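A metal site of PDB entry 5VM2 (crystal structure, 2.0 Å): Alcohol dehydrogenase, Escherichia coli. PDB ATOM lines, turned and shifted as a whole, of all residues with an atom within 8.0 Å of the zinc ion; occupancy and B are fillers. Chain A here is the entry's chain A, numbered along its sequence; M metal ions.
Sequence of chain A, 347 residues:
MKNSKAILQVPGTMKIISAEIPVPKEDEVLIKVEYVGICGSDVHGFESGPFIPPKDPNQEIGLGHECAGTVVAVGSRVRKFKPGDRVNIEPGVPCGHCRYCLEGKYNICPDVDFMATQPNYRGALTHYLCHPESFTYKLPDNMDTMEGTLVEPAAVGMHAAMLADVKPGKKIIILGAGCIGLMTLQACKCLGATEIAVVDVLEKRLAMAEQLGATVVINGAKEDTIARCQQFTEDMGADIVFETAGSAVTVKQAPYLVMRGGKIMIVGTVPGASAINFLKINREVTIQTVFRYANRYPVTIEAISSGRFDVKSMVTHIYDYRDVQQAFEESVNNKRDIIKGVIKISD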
ATOM      1  N   VAL A  93     -20.956  13.128 -18.581  1.00  0.00           N
ATOM      2  CA  VAL A  93     -21.332  14.353 -19.278  1.00  0.00           C
ATOM      3  C   VAL A  93     -20.061  15.155 -19.520  1.00  0.00           C
ATOM      4  O   VAL A  93     -19.493  15.713 -18.561  1.00  0.00           O
ATOM      5  CB  VAL A  93     -22.351  15.170 -18.470  1.00  0.00           C
ATOM      6  CG1 VAL A  93     -22.699  16.464 -19.205  1.00  0.00           C
ATOM      7  CG2 VAL A  93     -23.593  14.335 -18.172  1.00  0.00           C
ATOM      8  N   PRO A  94     -19.576  15.258 -20.762  1.00  0.00           N
ATOM      9  CA  PRO A  94     -18.302  15.913 -21.018  1.00  0.00           C
ATOM     10  C   PRO A  94     -18.479  17.427 -21.118  1.00  0.00           C
ATOM     11  O   PRO A  94     -19.589  17.951 -21.110  1.00  0.00           O
ATOM     12  CB  PRO A  94     -17.887  15.323 -22.360  1.00  0.00           C
ATOM     13  CG  PRO A  94     -19.207  15.188 -23.074  1.00  0.00           C
ATOM     14  CD  PRO A  94     -20.247  14.852 -22.005  1.00  0.00           C
ATOM     15  N   CYS A  95     -17.345  18.130 -21.220  1.00  0.00           N
ATOM     16  CA  CYS A  95     -17.391  19.585 -21.189  1.00  0.00           C
ATOM     17  C   CYS A  95     -17.928  20.171 -22.493  1.00  0.00           C
ATOM     18  O   CYS A  95     -18.534  21.243 -22.471  1.00  0.00           O
ATOM     19  CB  CYS A  95     -16.008  20.156 -20.851  1.00  0.00           C
ATOM     20  SG  CYS A  95     -14.834  20.428 -22.226  1.00  0.00           S
ATOM     21  N   GLY A  96     -17.733  19.474 -23.623  1.00  0.00           N
ATOM     22  CA  GLY A  96     -18.270  19.921 -24.898  1.00  0.00           C
ATOM     23  C   GLY A  96     -17.441  20.941 -25.651  1.00  0.00           C
ATOM     24  O   GLY A  96     -17.808  21.284 -26.787  1.00  0.00           O
ATOM     25  N   HIS A  97     -16.348  21.450 -25.078  1.00  0.00           N
ATOM     26  CA  HIS A  97     -15.576  22.503 -25.733  1.00  0.00           C
ATOM     27  C   HIS A  97     -14.072  22.263 -25.784  1.00  0.00           C
ATOM     28  O   HIS A  97     -13.366  23.053 -26.423  1.00  0.00           O
ATOM     29  CB  HIS A  97     -15.838  23.862 -25.066  1.00  0.00           C
ATOM     30  CG  HIS A  97     -15.456  23.901 -23.617  1.00  0.00           C
ATOM     31  ND1 HIS A  97     -14.150  23.992 -23.186  1.00  0.00           N
ATOM     32  CD2 HIS A  97     -16.222  23.857 -22.491  1.00  0.00           C
ATOM     33  CE1 HIS A  97     -14.121  24.017 -21.865  1.00  0.00           C
ATOM     34  NE2 HIS A  97     -15.362  23.929 -21.415  1.00  0.00           N
ATOM     35  N   CYS A  98     -13.552  21.226 -25.132  1.00  0.00           N
ATOM     36  CA  CYS A  98     -12.123  20.990 -25.161  1.00  0.00           C
ATOM     37  C   CYS A  98     -11.731  20.296 -26.471  1.00  0.00           C
ATOM     38  O   CYS A  98     -12.577  19.894 -27.272  1.00  0.00           O
ATOM     39  CB  CYS A  98     -11.685  20.147 -23.955  1.00  0.00           C
ATOM     40  SG  CYS A  98     -12.127  18.400 -24.039  1.00  0.00           S
ATOM     41  N   ARG A  99     -10.407  20.167 -26.677  1.00  0.00           N
ATOM     42  CA  ARG A  99      -9.910  19.557 -27.903  1.00  0.00           C
ATOM     43  C   ARG A  99     -10.427  18.132 -28.079  1.00  0.00           C
ATOM     44  O   ARG A  99     -10.683  17.698 -29.212  1.00  0.00           O
ATOM     45  CB  ARG A  99      -8.372  19.581 -27.926  1.00  0.00           C
ATOM     46  CG  ARG A  99      -7.707  18.346 -27.319  1.00  0.00           C
ATOM     47  CD  ARG A  99      -6.233  18.553 -27.016  1.00  0.00           C
ATOM     48  NE  ARG A  99      -5.353  18.347 -28.179  1.00  0.00           N
ATOM     49  CZ  ARG A  99      -5.192  17.198 -28.821  1.00  0.00           C
ATOM     50  NH1 ARG A  99      -5.850  16.113 -28.446  1.00  0.00           N
ATOM     51  NH2 ARG A  99      -4.359  17.128 -29.848  1.00  0.00           N
ATOM     52  N   TYR A 100     -10.606  17.380 -26.985  1.00  0.00           N
ATOM     53  CA  TYR A 100     -11.039  15.998 -27.131  1.00  0.00           C
ATOM     54  C   TYR A 100     -12.525  15.900 -27.444  1.00  0.00           C
ATOM     55  O   TYR A 100     -12.926  15.057 -28.252  1.00  0.00           O
ATOM     56  CB  TYR A 100     -10.699  15.203 -25.871  1.00  0.00           C
ATOM     57  CG  TYR A 100      -9.272  15.378 -25.454  1.00  0.00           C
ATOM     58  CD1 TYR A 100      -8.239  14.734 -26.123  1.00  0.00           C
ATOM     59  CD2 TYR A 100      -8.937  16.222 -24.407  1.00  0.00           C
ATOM     60  CE1 TYR A 100      -6.923  14.904 -25.740  1.00  0.00           C
ATOM     61  CE2 TYR A 100      -7.624  16.404 -24.017  1.00  0.00           C
ATOM     62  CZ  TYR A 100      -6.625  15.744 -24.686  1.00  0.00           C
ATOM     63  OH  TYR A 100      -5.319  15.929 -24.290  1.00  0.00           O
ATOM     64  N   CYS A 101     -13.344  16.741 -26.807  1.00  0.00           N
ATOM     65  CA  CYS A 101     -14.764  16.770 -27.144  1.00  0.00           C
ATOM     66  C   CYS A 101     -14.953  17.185 -28.593  1.00  0.00           C
ATOM     67  O   CYS A 101     -15.730  16.558 -29.332  1.00  0.00           O
ATOM     68  CB  CYS A 101     -15.503  17.733 -26.219  1.00  0.00           C
ATOM     69  SG  CYS A 101     -15.677  17.124 -24.535  1.00  0.00           S
ATOM     70  N   LEU A 102     -14.262  18.236 -29.026  1.00  0.00           N
ATOM     71  CA  LEU A 102     -14.400  18.729 -30.386  1.00  0.00           C
ATOM     72  C   LEU A 102     -13.830  17.777 -31.428  1.00  0.00           C
ATOM     73  O   LEU A 102     -14.180  17.898 -32.605  1.00  0.00           O
ATOM     74  CB  LEU A 102     -13.719  20.097 -30.518  1.00  0.00           C
ATOM     75  CG  LEU A 102     -14.429  21.260 -29.825  1.00  0.00           C
ATOM     76  CD1 LEU A 102     -13.705  22.573 -30.093  1.00  0.00           C
ATOM     77  CD2 LEU A 102     -15.878  21.349 -30.267  1.00  0.00           C
ATOM     78  N   LYS A 105     -13.761  12.560 -29.221  1.00  0.00           N
ATOM     79  CA  LYS A 105     -13.324  11.695 -28.123  1.00  0.00           C
ATOM     80  C   LYS A 105     -13.782  12.251 -26.782  1.00  0.00           C
ATOM     81  O   LYS A 105     -13.004  12.286 -25.822  1.00  0.00           O
ATOM     82  CB  LYS A 105     -11.807  11.523 -28.129  1.00  0.00           C
ATOM     83  CG  LYS A 105     -11.215  10.720 -29.295  1.00  0.00           C
ATOM     84  CD  LYS A 105      -9.691  10.666 -29.156  1.00  0.00           C
ATOM     85  CE  LYS A 105      -9.013   9.918 -30.313  1.00  0.00           C
ATOM     86  NZ  LYS A 105      -7.519  10.046 -30.229  1.00  0.00           N
ATOM     87  N   TYR A 106     -15.040  12.685 -26.686  1.00  0.00           N
ATOM     88  CA  TYR A 106     -15.494  13.292 -25.437  1.00  0.00           C
ATOM     89  C   TYR A 106     -15.323  12.377 -24.237  1.00  0.00           C
ATOM     90  O   TYR A 106     -15.274  12.853 -23.099  1.00  0.00           O
ATOM     91  CB  TYR A 106     -16.961  13.747 -25.566  1.00  0.00           C
ATOM     92  CG  TYR A 106     -18.025  12.650 -25.646  1.00  0.00           C
ATOM     93  CD1 TYR A 106     -18.431  11.958 -24.514  1.00  0.00           C
ATOM     94  CD2 TYR A 106     -18.657  12.356 -26.854  1.00  0.00           C
ATOM     95  CE1 TYR A 106     -19.410  10.975 -24.586  1.00  0.00           C
ATOM     96  CE2 TYR A 106     -19.641  11.364 -26.927  1.00  0.00           C
ATOM     97  CZ  TYR A 106     -20.013  10.676 -25.789  1.00  0.00           C
ATOM     98  OH  TYR A 106     -20.992   9.701 -25.832  1.00  0.00           O
ATOM     99  N   ASN A 107     -15.202  11.059 -24.455  1.00  0.00           N
ATOM    100  CA  ASN A 107     -15.053  10.140 -23.331  1.00  0.00           C
ATOM    101  C   ASN A 107     -13.777  10.395 -22.553  1.00  0.00           C
ATOM    102  O   ASN A 107     -13.720  10.120 -21.350  1.00  0.00           O
ATOM    103  CB  ASN A 107     -15.109   8.682 -23.811  1.00  0.00           C
ATOM    104  CG  ASN A 107     -14.079   8.375 -24.883  1.00  0.00           C
ATOM    105  OD1 ASN A 107     -13.911   9.141 -25.828  1.00  0.00           O
ATOM    106  ND2 ASN A 107     -13.419   7.225 -24.759  1.00  0.00           N
ATOM    107  N   ILE A 108     -12.738  10.907 -23.211  1.00  0.00           N
ATOM    108  CA  ILE A 108     -11.487  11.207 -22.524  1.00  0.00           C
ATOM    109  C   ILE A 108     -11.397  12.680 -22.144  1.00  0.00           C
ATOM    110  O   ILE A 108     -10.301  13.168 -21.830  1.00  0.00           O
ATOM    111  CB  ILE A 108     -10.260  10.759 -23.351  1.00  0.00           C
ATOM    112  CG1 ILE A 108     -10.073  11.646 -24.580  1.00  0.00           C
ATOM    113  CG2 ILE A 108     -10.394   9.301 -23.760  1.00  0.00           C
ATOM    114  CD1 ILE A 108      -8.921  11.188 -25.479  1.00  0.00           C
ATOM    115  N   CYS A 109     -12.508  13.400 -22.165  1.00  0.00           N
ATOM    116  CA  CYS A 109     -12.555  14.796 -21.760  1.00  0.00           C
ATOM    117  C   CYS A 109     -11.998  14.950 -20.344  1.00  0.00           C
ATOM    118  O   CYS A 109     -12.431  14.226 -19.432  1.00  0.00           O
ATOM    119  CB  CYS A 109     -13.986  15.326 -21.817  1.00  0.00           C
ATOM    120  SG  CYS A 109     -14.241  16.983 -21.091  1.00  0.00           S
ATOM    121  N   PRO A 110     -11.038  15.860 -20.117  1.00  0.00           N
ATOM    122  CA  PRO A 110     -10.468  16.014 -18.770  1.00  0.00           C
ATOM    123  C   PRO A 110     -11.443  16.593 -17.753  1.00  0.00           C
ATOM    124  O   PRO A 110     -11.167  16.509 -16.553  1.00  0.00           O
ATOM    125  CB  PRO A 110      -9.287  16.954 -19.000  1.00  0.00           C
ATOM    126  CG  PRO A 110      -9.673  17.745 -20.196  1.00  0.00           C
ATOM    127  CD  PRO A 110     -10.470  16.813 -21.076  1.00  0.00           C
ATOM    128  N   ASP A 111     -12.561  17.165 -18.192  1.00  0.00           N
ATOM    129  CA  ASP A 111     -13.560  17.723 -17.294  1.00  0.00           C
ATOM    130  C   ASP A 111     -14.897  16.992 -17.416  1.00  0.00           C
ATOM    131  O   ASP A 111     -15.955  17.611 -17.275  1.00  0.00           O
ATOM    132  CB  ASP A 111     -13.747  19.213 -17.547  1.00  0.00           C
ATOM    133  CG  ASP A 111     -12.534  20.029 -17.153  1.00  0.00           C
ATOM    134  OD1 ASP A 111     -12.042  19.870 -16.014  1.00  0.00           O
ATOM    135  OD2 ASP A 111     -12.067  20.841 -17.986  1.00  0.00           O
ATOM    136  N   VAL A 112     -14.868  15.683 -17.686  1.00  0.00           N
ATOM    137  CA  VAL A 112     -16.110  14.916 -17.719  1.00  0.00           C
ATOM    138  C   VAL A 112     -16.699  14.841 -16.317  1.00  0.00           C
ATOM    139  O   VAL A 112     -15.978  14.710 -15.317  1.00  0.00           O
ATOM    140  CB  VAL A 112     -15.880  13.510 -18.313  1.00  0.00           C
ATOM    141  CG1 VAL A 112     -14.962  12.680 -17.416  1.00  0.00           C
ATOM    142  CG2 VAL A 112     -17.213  12.795 -18.506  1.00  0.00           C
HETATM  143 ZN    ZN M   1     -14.211  18.270 -22.987  1.00  0.00          ZN
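Gly 96 touches the zinc ion.
Of the 18 residues printed, 5 come within 4 Å of the zinc ion.
The nearest printed residue that does not touch the zinc ion is His 97 (4.4 Å).
SG of Cys 109 binds the zinc ion, at 2.3 Å.
The zinc ion is bound by SG of Cys 98, at 2.3 Å.
The side-chain sulfur (SG) of Cys 95 is bound to the zinc ion (2.4 Å).
The zinc ion is bound by SG of Cys 101, at 2.4 Å.
The zinc ion has four donor atoms within binding distance.
The side-chain sulfur (SG) of Cys 95 sits close to the backbone NH (N) of His 97, at 3.4 Å.
The side-chain sulfur of Cys 109 sits close to the backbone NH of Val 112 (3.7 Å).
The side-chain sulfur (SG) of Cys 101 lies close to the backbone NH (N) of Gly 96 (3.3 Å).
N of Asp 111 sits close to SG of Cys 109, 3.4 Å away.
SG of Cys 98 sits close to N of Tyr 100 (3.5 Å).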
